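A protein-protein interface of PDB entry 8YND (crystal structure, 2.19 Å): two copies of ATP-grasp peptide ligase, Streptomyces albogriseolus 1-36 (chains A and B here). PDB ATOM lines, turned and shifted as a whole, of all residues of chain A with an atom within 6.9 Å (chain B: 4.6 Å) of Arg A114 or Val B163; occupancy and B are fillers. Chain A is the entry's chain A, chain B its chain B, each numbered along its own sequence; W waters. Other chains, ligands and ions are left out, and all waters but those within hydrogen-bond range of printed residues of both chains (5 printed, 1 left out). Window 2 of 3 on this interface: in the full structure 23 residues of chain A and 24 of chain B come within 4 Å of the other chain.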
ATOM      1  N   GLU A  83     -19.202  15.234   8.244  1.00  0.00           N
ATOM      2  CA  GLU A  83     -18.211  15.898   9.081  1.00  0.00           C
ATOM      3  C   GLU A  83     -18.842  17.076   9.814  1.00  0.00           C
ATOM      4  O   GLU A  83     -18.560  17.309  11.001  1.00  0.00           O
ATOM      5  CB  GLU A  83     -17.020  16.363   8.237  1.00  0.00           C
ATOM      6  CG  GLU A  83     -16.173  15.245   7.637  1.00  0.00           C
ATOM      7  CD  GLU A  83     -15.412  14.417   8.663  1.00  0.00           C
ATOM      8  OE1 GLU A  83     -15.970  13.415   9.192  1.00  0.00           O
ATOM      9  OE2 GLU A  83     -14.230  14.762   8.922  1.00  0.00           O
ATOM     10  N   LEU A  86     -20.489  15.750  12.942  1.00  0.00           N
ATOM     11  CA  LEU A  86     -19.533  15.379  13.976  1.00  0.00           C
ATOM     12  C   LEU A  86     -18.878  16.592  14.617  1.00  0.00           C
ATOM     13  O   LEU A  86     -18.326  16.473  15.715  1.00  0.00           O
ATOM     14  CB  LEU A  86     -18.450  14.479  13.382  1.00  0.00           C
ATOM     15  CG  LEU A  86     -18.848  13.185  12.666  1.00  0.00           C
ATOM     16  CD1 LEU A  86     -17.596  12.335  12.389  1.00  0.00           C
ATOM     17  CD2 LEU A  86     -19.882  12.384  13.452  1.00  0.00           C
ATOM     18  N   GLN A  87     -18.871  17.731  13.918  1.00  0.00           N
ATOM     19  CA  GLN A  87     -18.401  19.014  14.420  1.00  0.00           C
ATOM     20  C   GLN A  87     -19.483  19.767  15.182  1.00  0.00           C
ATOM     21  O   GLN A  87     -19.160  20.655  15.980  1.00  0.00           O
ATOM     22  CB  GLN A  87     -17.932  19.891  13.241  1.00  0.00           C
ATOM     23  CG  GLN A  87     -16.587  19.496  12.616  1.00  0.00           C
ATOM     24  CD  GLN A  87     -15.386  20.006  13.405  1.00  0.00           C
ATOM     25  OE1 GLN A  87     -14.663  20.910  12.960  1.00  0.00           O
ATOM     26  NE2 GLN A  87     -15.187  19.448  14.596  1.00  0.00           N
ATOM     27  N   VAL A 111     -15.282   5.443   9.487  1.00  0.00           N
ATOM     28  CA  VAL A 111     -14.289   6.112   8.662  1.00  0.00           C
ATOM     29  C   VAL A 111     -13.512   7.030   9.592  1.00  0.00           C
ATOM     30  O   VAL A 111     -14.112   7.853  10.293  1.00  0.00           O
ATOM     31  CB  VAL A 111     -14.943   6.908   7.513  1.00  0.00           C
ATOM     32  CG1 VAL A 111     -13.914   7.471   6.592  1.00  0.00           C
ATOM     33  CG2 VAL A 111     -15.893   6.037   6.701  1.00  0.00           C
ATOM     34  N   SER A 112     -12.191   6.872   9.637  1.00  0.00           N
ATOM     35  CA  SER A 112     -11.391   7.662  10.567  1.00  0.00           C
ATOM     36  C   SER A 112     -11.102   9.033   9.946  1.00  0.00           C
ATOM     37  O   SER A 112      -9.990   9.350   9.516  1.00  0.00           O
ATOM     38  CB  SER A 112     -10.115   6.926  10.939  1.00  0.00           C
ATOM     39  OG  SER A 112     -10.335   6.035  12.025  1.00  0.00           O
ATOM     40  N   THR A 113     -12.135   9.865   9.918  1.00  0.00           N
ATOM     41  CA  THR A 113     -11.973  11.187   9.350  1.00  0.00           C
ATOM     42  C   THR A 113     -11.391  12.167  10.367  1.00  0.00           C
ATOM     43  O   THR A 113     -11.305  11.894  11.559  1.00  0.00           O
ATOM     44  CB  THR A 113     -13.308  11.721   8.875  1.00  0.00           C
ATOM     45  OG1 THR A 113     -14.152  11.929  10.020  1.00  0.00           O
ATOM     46  CG2 THR A 113     -13.959  10.725   7.950  1.00  0.00           C
ATOM     47  N   ARG A 114     -11.036  13.347   9.866  1.00  0.00           N
ATOM     48  CA  ARG A 114     -10.556  14.432  10.710  1.00  0.00           C
ATOM     49  C   ARG A 114     -11.575  14.805  11.776  1.00  0.00           C
ATOM     50  O   ARG A 114     -11.217  15.039  12.931  1.00  0.00           O
ATOM     51  CB  ARG A 114     -10.234  15.646   9.845  1.00  0.00           C
ATOM     52  CG  ARG A 114      -9.936  16.900  10.622  1.00  0.00           C
ATOM     53  CD  ARG A 114      -9.590  18.022   9.670  1.00  0.00           C
ATOM     54  NE  ARG A 114      -9.433  19.279  10.378  1.00  0.00           N
ATOM     55  CZ  ARG A 114      -8.295  19.678  10.927  1.00  0.00           C
ATOM     56  NH1 ARG A 114      -7.223  18.910  10.920  1.00  0.00           N
ATOM     57  NH2 ARG A 114      -8.228  20.887  11.480  1.00  0.00           N
ATOM     58  N   ALA A 115     -12.848  14.891  11.404  1.00  0.00           N
ATOM     59  CA  ALA A 115     -13.856  15.203  12.407  1.00  0.00           C
ATOM     60  C   ALA A 115     -13.997  14.082  13.424  1.00  0.00           C
ATOM     61  O   ALA A 115     -14.244  14.353  14.604  1.00  0.00           O
ATOM     62  CB  ALA A 115     -15.199  15.488  11.745  1.00  0.00           C
ATOM     63  N   ALA A 116     -13.829  12.826  13.001  1.00  0.00           N
ATOM     64  CA  ALA A 116     -13.904  11.724  13.956  1.00  0.00           C
ATOM     65  C   ALA A 116     -12.785  11.818  14.981  1.00  0.00           C
ATOM     66  O   ALA A 116     -13.007  11.580  16.178  1.00  0.00           O
ATOM     67  CB  ALA A 116     -13.855  10.372  13.237  1.00  0.00           C
ATOM     68  N   ALA A 117     -11.573  12.169  14.527  1.00  0.00           N
ATOM     69  CA  ALA A 117     -10.457  12.319  15.451  1.00  0.00           C
ATOM     70  C   ALA A 117     -10.658  13.542  16.331  1.00  0.00           C
ATOM     71  O   ALA A 117     -10.405  13.497  17.540  1.00  0.00           O
ATOM     72  CB  ALA A 117      -9.135  12.410  14.684  1.00  0.00           C
ATOM     73  N   GLN A 118     -11.119  14.641  15.733  1.00  0.00           N
ATOM     74  CA  GLN A 118     -11.528  15.799  16.519  1.00  0.00           C
ATOM     75  C   GLN A 118     -12.542  15.412  17.587  1.00  0.00           C
ATOM     76  O   GLN A 118     -12.433  15.849  18.738  1.00  0.00           O
ATOM     77  CB  GLN A 118     -12.106  16.874  15.595  1.00  0.00           C
ATOM     78  CG  GLN A 118     -11.026  17.633  14.835  1.00  0.00           C
ATOM     79  CD  GLN A 118     -11.576  18.652  13.860  1.00  0.00           C
ATOM     80  OE1 GLN A 118     -12.573  18.414  13.180  1.00  0.00           O
ATOM     81  NE2 GLN A 118     -10.912  19.801  13.779  1.00  0.00           N
ATOM     82  N   LEU A 119     -13.537  14.591  17.220  1.00  0.00           N
ATOM     83  CA  LEU A 119     -14.586  14.199  18.167  1.00  0.00           C
ATOM     84  C   LEU A 119     -14.000  13.542  19.413  1.00  0.00           C
ATOM     85  O   LEU A 119     -14.413  13.849  20.538  1.00  0.00           O
ATOM     86  CB  LEU A 119     -15.569  13.256  17.492  1.00  0.00           C
ATOM     87  CG  LEU A 119     -16.886  12.962  18.201  1.00  0.00           C
ATOM     88  CD1 LEU A 119     -17.588  14.252  18.631  1.00  0.00           C
ATOM     89  CD2 LEU A 119     -17.794  12.123  17.270  1.00  0.00           C
ATOM     90  N   LEU A 128      -8.373   8.584  19.176  1.00  0.00           N
ATOM     91  CA  LEU A 128      -8.414   7.758  17.981  1.00  0.00           C
ATOM     92  C   LEU A 128      -7.014   7.273  17.612  1.00  0.00           C
ATOM     93  O   LEU A 128      -6.055   8.057  17.564  1.00  0.00           O
ATOM     94  CB  LEU A 128      -9.020   8.558  16.831  1.00  0.00           C
ATOM     95  CG  LEU A 128      -9.322   7.774  15.554  1.00  0.00           C
ATOM     96  CD1 LEU A 128     -10.752   7.349  15.532  1.00  0.00           C
ATOM     97  CD2 LEU A 128      -8.999   8.593  14.319  1.00  0.00           C
ATOM     98  N   TYR A 131      -4.347   9.169  15.115  1.00  0.00           N
ATOM     99  CA  TYR A 131      -4.965  10.482  15.215  1.00  0.00           C
ATOM    100  C   TYR A 131      -4.333  11.473  14.241  1.00  0.00           C
ATOM    101  O   TYR A 131      -5.033  12.100  13.435  1.00  0.00           O
ATOM    102  CB  TYR A 131      -4.849  10.961  16.663  1.00  0.00           C
ATOM    103  CG  TYR A 131      -5.292  12.376  16.944  1.00  0.00           C
ATOM    104  CD1 TYR A 131      -6.617  12.655  17.291  1.00  0.00           C
ATOM    105  CD2 TYR A 131      -4.379  13.443  16.897  1.00  0.00           C
ATOM    106  CE1 TYR A 131      -7.027  13.949  17.566  1.00  0.00           C
ATOM    107  CE2 TYR A 131      -4.784  14.748  17.178  1.00  0.00           C
ATOM    108  CZ  TYR A 131      -6.110  14.992  17.516  1.00  0.00           C
ATOM    109  OH  TYR A 131      -6.525  16.278  17.794  1.00  0.00           O
ATOM    110  N   PHE A 133      -2.602  11.071  11.605  1.00  0.00           N
ATOM    111  CA  PHE A 133      -2.896  10.707  10.224  1.00  0.00           C
ATOM    112  C   PHE A 133      -4.279  11.196   9.829  1.00  0.00           C
ATOM    113  O   PHE A 133      -4.454  11.855   8.793  1.00  0.00           O
ATOM    114  CB  PHE A 133      -2.783   9.184  10.057  1.00  0.00           C
ATOM    115  CG  PHE A 133      -2.827   8.703   8.602  1.00  0.00           C
ATOM    116  CD1 PHE A 133      -1.813   9.045   7.700  1.00  0.00           C
ATOM    117  CD2 PHE A 133      -3.870   7.894   8.156  1.00  0.00           C
ATOM    118  CE1 PHE A 133      -1.840   8.591   6.384  1.00  0.00           C
ATOM    119  CE2 PHE A 133      -3.910   7.425   6.839  1.00  0.00           C
ATOM    120  CZ  PHE A 133      -2.895   7.776   5.948  1.00  0.00           C
ATOM    121  N   ALA A 134      -5.277  10.893  10.663  1.00  0.00           N
ATOM    122  CA  ALA A 134      -6.651  11.300  10.387  1.00  0.00           C
ATOM    123  C   ALA A 134      -6.808  12.818  10.431  1.00  0.00           C
ATOM    124  O   ALA A 134      -7.581  13.381   9.661  1.00  0.00           O
ATOM    125  CB  ALA A 134      -7.592  10.630  11.390  1.00  0.00           C
ATOM    126  N   MET A 135      -6.112  13.489  11.350  1.00  0.00           N
ATOM    127  CA  MET A 135      -6.134  14.949  11.401  1.00  0.00           C
ATOM    128  C   MET A 135      -5.747  15.574  10.057  1.00  0.00           C
ATOM    129  O   MET A 135      -6.276  16.631   9.690  1.00  0.00           O
ATOM    130  CB  MET A 135      -5.200  15.412  12.526  1.00  0.00           C
ATOM    131  CG  MET A 135      -5.821  15.553  13.927  1.00  0.00           C
ATOM    132  SD  MET A 135      -7.567  16.032  13.995  1.00  0.00           S
ATOM    133  CE  MET A 135      -7.359  17.784  14.283  1.00  0.00           C
ATOM    134  N   GLN A 136      -4.851  14.939   9.298  1.00  0.00           N
ATOM    135  CA  GLN A 136      -4.505  15.399   7.956  1.00  0.00           C
ATOM    136  C   GLN A 136      -5.394  14.794   6.867  1.00  0.00           C
ATOM    137  O   GLN A 136      -5.069  14.909   5.672  1.00  0.00           O
ATOM    138  CB  GLN A 136      -3.039  15.091   7.654  1.00  0.00           C
ATOM    139  CG  GLN A 136      -2.042  15.711   8.616  1.00  0.00           C
ATOM    140  CD  GLN A 136      -2.210  17.200   8.730  1.00  0.00           C
ATOM    141  OE1 GLN A 136      -2.078  17.910   7.737  1.00  0.00           O
ATOM    142  NE2 GLN A 136      -2.477  17.695   9.949  1.00  0.00           N
ATOM    143  N   ASN A 137      -6.512  14.176   7.259  1.00  0.00           N
ATOM    144  CA  ASN A 137      -7.383  13.410   6.365  1.00  0.00           C
ATOM    145  C   ASN A 137      -6.582  12.422   5.523  1.00  0.00           C
ATOM    146  O   ASN A 137      -6.757  12.305   4.306  1.00  0.00           O
ATOM    147  CB  ASN A 137      -8.237  14.334   5.491  1.00  0.00           C
ATOM    148  CG  ASN A 137      -9.377  14.968   6.279  1.00  0.00           C
ATOM    149  OD1 ASN A 137     -10.277  14.270   6.791  1.00  0.00           O
ATOM    150  ND2 ASN A 137      -9.324  16.287   6.418  1.00  0.00           N
ATOM    151  N   GLY A 138      -5.715  11.684   6.211  1.00  0.00           N
ATOM    152  CA  GLY A 138      -4.909  10.690   5.541  1.00  0.00           C
ATOM    153  C   GLY A 138      -5.741   9.656   4.827  1.00  0.00           C
ATOM    154  O   GLY A 138      -5.355   9.186   3.755  1.00  0.00           O
ATOM    155  N   ILE A 139      -6.895   9.293   5.395  1.00  0.00           N
ATOM    156  CA  ILE A 139      -7.618   8.165   4.829  1.00  0.00           C
ATOM    157  C   ILE A 139      -8.372   8.577   3.570  1.00  0.00           C
ATOM    158  O   ILE A 139      -8.741   7.710   2.769  1.00  0.00           O
ATOM    159  CB  ILE A 139      -8.526   7.491   5.879  1.00  0.00           C
ATOM    160  CG1 ILE A 139      -9.795   8.282   6.113  1.00  0.00           C
ATOM    161  CG2 ILE A 139      -7.791   7.261   7.207  1.00  0.00           C
ATOM    162  CD1 ILE A 139     -10.891   7.734   5.346  1.00  0.00           C
ATOM    163  N   ARG B 149       2.295  15.959   4.262  1.00  0.00           N
ATOM    164  CA  ARG B 149       1.682  16.098   5.584  1.00  0.00           C
ATOM    165  C   ARG B 149       1.063  14.781   6.048  1.00  0.00           C
ATOM    166  O   ARG B 149       1.230  14.377   7.210  1.00  0.00           O
ATOM    167  CB  ARG B 149       0.625  17.210   5.542  1.00  0.00           C
ATOM    168  CG  ARG B 149       1.253  18.647   5.432  1.00  0.00           C
ATOM    169  CD  ARG B 149       0.396  19.743   6.102  1.00  0.00           C
ATOM    170  NE  ARG B 149       0.176  19.478   7.525  1.00  0.00           N
ATOM    171  CZ  ARG B 149       0.977  19.866   8.514  1.00  0.00           C
ATOM    172  NH1 ARG B 149       2.047  20.623   8.294  1.00  0.00           N
ATOM    173  NH2 ARG B 149       0.686  19.502   9.760  1.00  0.00           N
ATOM    174  N   GLY B 162      -0.469  22.023  11.144  1.00  0.00           N
ATOM    175  CA  GLY B 162      -0.988  22.494   9.879  1.00  0.00           C
ATOM    176  C   GLY B 162      -2.258  21.768   9.518  1.00  0.00           C
ATOM    177  O   GLY B 162      -2.641  20.781  10.154  1.00  0.00           O
ATOM    178  N   VAL B 163      -2.897  22.278   8.469  1.00  0.00           N
ATOM    179  CA  VAL B 163      -4.145  21.745   7.948  1.00  0.00           C
ATOM    180  C   VAL B 163      -4.000  21.541   6.442  1.00  0.00           C
ATOM    181  O   VAL B 163      -3.433  22.392   5.741  1.00  0.00           O
ATOM    182  CB  VAL B 163      -5.321  22.702   8.277  1.00  0.00           C
ATOM    183  CG1 VAL B 163      -6.604  22.273   7.597  1.00  0.00           C
ATOM    184  CG2 VAL B 163      -5.534  22.796   9.797  1.00  0.00           C
ATOM    185  N   VAL B 164      -4.509  20.410   5.945  1.00  0.00           N
ATOM    186  CA  VAL B 164      -4.797  20.236   4.522  1.00  0.00           C
ATOM    187  C   VAL B 164      -6.181  20.812   4.265  1.00  0.00           C
ATOM    188  O   VAL B 164      -7.193  20.117   4.403  1.00  0.00           O
ATOM    189  CB  VAL B 164      -4.708  18.757   4.091  1.00  0.00           C
ATOM    190  CG1 VAL B 164      -5.190  18.558   2.644  1.00  0.00           C
ATOM    191  CG2 VAL B 164      -3.271  18.241   4.236  1.00  0.00           C
ATOM    192  N   ALA B 165      -6.223  22.095   3.906  1.00  0.00           N
ATOM    193  CA  ALA B 165      -7.462  22.834   3.726  1.00  0.00           C
ATOM    194  C   ALA B 165      -8.205  22.433   2.448  1.00  0.00           C
ATOM    195  O   ALA B 165      -7.610  22.282   1.376  1.00  0.00           O
ATOM    196  CB  ALA B 165      -7.166  24.335   3.690  1.00  0.00           C
ATOM    197  N   ARG B 166      -9.533  22.314   2.553  1.00  0.00           N
ATOM    198  CA  ARG B 166     -10.366  21.888   1.439  1.00  0.00           C
ATOM    199  C   ARG B 166     -11.301  22.973   0.914  1.00  0.00           C
ATOM    200  O   ARG B 166     -11.933  22.768  -0.134  1.00  0.00           O
ATOM    201  CB  ARG B 166     -11.189  20.655   1.841  1.00  0.00           C
ATOM    202  CG  ARG B 166     -10.314  19.427   2.107  1.00  0.00           C
ATOM    203  CD  ARG B 166     -11.028  18.314   2.882  1.00  0.00           C
ATOM    204  NE  ARG B 166     -11.325  18.692   4.259  1.00  0.00           N
ATOM    205  CZ  ARG B 166     -11.942  17.903   5.127  1.00  0.00           C
ATOM    206  NH1 ARG B 166     -12.337  16.686   4.784  1.00  0.00           N
ATOM    207  NH2 ARG B 166     -12.156  18.341   6.376  1.00  0.00           N
ATOM    208  N   GLU B 170     -12.389  26.375   5.479  1.00  0.00           N
ATOM    209  CA  GLU B 170     -11.323  25.683   6.188  1.00  0.00           C
ATOM    210  C   GLU B 170     -10.016  26.479   6.162  1.00  0.00           C
ATOM    211  O   GLU B 170      -9.273  26.467   7.150  1.00  0.00           O
ATOM    212  CB  GLU B 170     -11.145  24.279   5.609  1.00  0.00           C
ATOM    213  CG  GLU B 170     -10.511  23.316   6.594  1.00  0.00           C
ATOM    214  CD  GLU B 170     -10.665  21.828   6.224  1.00  0.00           C
ATOM    215  OE1 GLU B 170     -10.771  21.476   5.025  1.00  0.00           O
ATOM    216  OE2 GLU B 170     -10.649  21.007   7.172  1.00  0.00           O
ATOM    217  N   ALA B 174      -8.395  27.422   9.832  1.00  0.00           N
ATOM    218  CA  ALA B 174      -6.986  27.057   9.934  1.00  0.00           C
ATOM    219  C   ALA B 174      -6.144  28.259  10.333  1.00  0.00           C
ATOM    220  O   ALA B 174      -5.344  28.190  11.274  1.00  0.00           O
ATOM    221  CB  ALA B 174      -6.497  26.476   8.605  1.00  0.00           C
ATOM    222  N   LEU B 178      -4.131  28.472  13.825  1.00  0.00           N
ATOM    223  CA  LEU B 178      -2.698  28.283  13.671  1.00  0.00           C
ATOM    224  C   LEU B 178      -1.902  29.557  13.918  1.00  0.00           C
ATOM    225  O   LEU B 178      -0.685  29.479  14.124  1.00  0.00           O
ATOM    226  CB  LEU B 178      -2.404  27.731  12.271  1.00  0.00           C
ATOM    227  CG  LEU B 178      -3.052  26.363  12.038  1.00  0.00           C
ATOM    228  CD1 LEU B 178      -2.771  25.881  10.636  1.00  0.00           C
ATOM    229  CD2 LEU B 178      -2.605  25.328  13.081  1.00  0.00           C
ATOM    230  N   ILE B 242      -5.318  23.290  -0.394  1.00  0.00           N
ATOM    231  CA  ILE B 242      -4.329  24.230   0.104  1.00  0.00           C
ATOM    232  C   ILE B 242      -3.740  23.644   1.370  1.00  0.00           C
ATOM    233  O   ILE B 242      -4.449  22.991   2.142  1.00  0.00           O
ATOM    234  CB  ILE B 242      -4.958  25.612   0.397  1.00  0.00           C
ATOM    235  CG1 ILE B 242      -5.548  26.185  -0.877  1.00  0.00           C
ATOM    236  CG2 ILE B 242      -3.941  26.590   0.972  1.00  0.00           C
ATOM    237  CD1 ILE B 242      -4.570  26.119  -2.005  1.00  0.00           C
ATOM    238  N   THR B 243      -2.457  23.888   1.592  1.00  0.00           N
ATOM    239  CA  THR B 243      -1.835  23.619   2.871  1.00  0.00           C
ATOM    240  C   THR B 243      -1.755  24.941   3.636  1.00  0.00           C
ATOM    241  O   THR B 243      -1.528  25.997   3.040  1.00  0.00           O
ATOM    242  CB  THR B 243      -0.451  22.974   2.670  1.00  0.00           C
ATOM    243  OG1 THR B 243      -0.603  21.557   2.473  1.00  0.00           O
ATOM    244  CG2 THR B 243       0.432  23.177   3.842  1.00  0.00           C
ATOM    245  N   VAL B 244      -2.015  24.888   4.942  1.00  0.00           N
ATOM    246  CA  VAL B 244      -1.923  26.053   5.820  1.00  0.00           C
ATOM    247  C   VAL B 244      -1.198  25.590   7.068  1.00  0.00           C
ATOM    248  O   VAL B 244      -1.669  24.672   7.750  1.00  0.00           O
ATOM    249  CB  VAL B 244      -3.292  26.652   6.199  1.00  0.00           C
ATOM    250  CG1 VAL B 244      -3.105  27.909   7.042  1.00  0.00           C
ATOM    251  CG2 VAL B 244      -4.115  26.982   4.963  1.00  0.00           C
HETATM  252  O   HOH W   1     -11.154  21.986   9.927  1.00  0.00           O
HETATM  253  O   HOH W   2      -6.236  18.942   7.754  1.00  0.00           O
HETATM  254  O   HOH W   3      -8.672  19.387   6.393  1.00  0.00           O
HETATM  255  O   HOH W   4     -13.028  14.694   6.494  1.00  0.00           O
HETATM  256  O   HOH W   5     -13.506  17.498   8.410  1.00  0.00           O
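The backbone NH of Arg A114 sits close to the backbone carbonyl oxygen of Ala A134 (3.5 Å). The guanidinium group of Arg A114 is in hydrogen-bond range of the backbone carbonyl oxygen of Met A135, 2.8 Å away. N of Val B163 sits at hydrogen-bond distance from O of Val B244. NE of Arg B166 is in salt-bridge range of OE1 of Glu B170, at 2.9 Å. OD1 of Asn A137 sits at hydrogen-bond distance from N of Arg A114 (3.3 Å).
Of the 12 printed residues of chain B, 6 touch a printed residue of chain A. Hydrophobic or aromatic side chains of chain B that line the printed part of chain A: Val B163 and Val B164. Among the printed residues, Asp or Glu carboxylates within 4 Å of a Lys or Arg side-chain nitrogen of the other chain: Arg A114 with Glu B170 (3.8 Å).
The side-chain amide oxygen of Gln A136 is in hydrogen-bond range of the guanidinium group of Arg B149. NE2 of Gln A136 is in hydrogen-bond range of O of Gly B162 (3.1 Å). The side-chain amide nitrogen of Asn A137 lies close to the guanidinium group of Arg B166 (3.5 Å). The guanidinium group (NE) of Arg A114 lies within salt-bridge range of the side-chain carboxylate (OE2) of Glu B170.
Water W5 bridges NH2 of Arg B166 (2.6 Å) and OE2 of Glu A83 (2.9 Å). Water W3 lies within hydrogen-bond range of the backbone carbonyl oxygen (O) of Val B164 (2.6 Å), the side-chain carboxylate (OE2) of Glu B170 (2.7 Å), the side-chain amide nitrogen (ND2) of Asn A137 (3.2 Å) and the guanidinium group (NE) of Arg B166 (3.5 Å). Water W4 lies within hydrogen-bond range of OE2 of Glu A83 (2.7 Å), NH1 of Arg B166 (2.7 Å) and OD1 of Asn A137 (2.8 Å). Water W2 lies within hydrogen-bond range of the backbone NH (N) of Val B164, the backbone carbonyl oxygen (O) of Met A135 and the guanidinium group (NH1) of Arg A114. Water W1 bridges OE2 of Glu B170 and NE of Arg A114.
NH2 of Arg A114 touches CG2 of Val B163, 3.7 Å away. Gln A136 touches Val B164 (OE1 to CG2, 3.7 Å).
Of chain B, only Val B163 and Glu B170 come within 4 Å of Arg A114. Of the printed residues of chain A, Arg B149 touches Gln A136. Val B163 touches just one residue of chain A: Arg A114 (3.7 Å). Of the printed residues of chain A, Val B164 touches Gln A136 (3.7 Å). Of the printed residues of chain A, Glu B170 touches Arg A114. The nearest printed residue of chain A that does not touch Gly B162 is Arg A114 (5.0 Å).
No position is printed for both chains.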
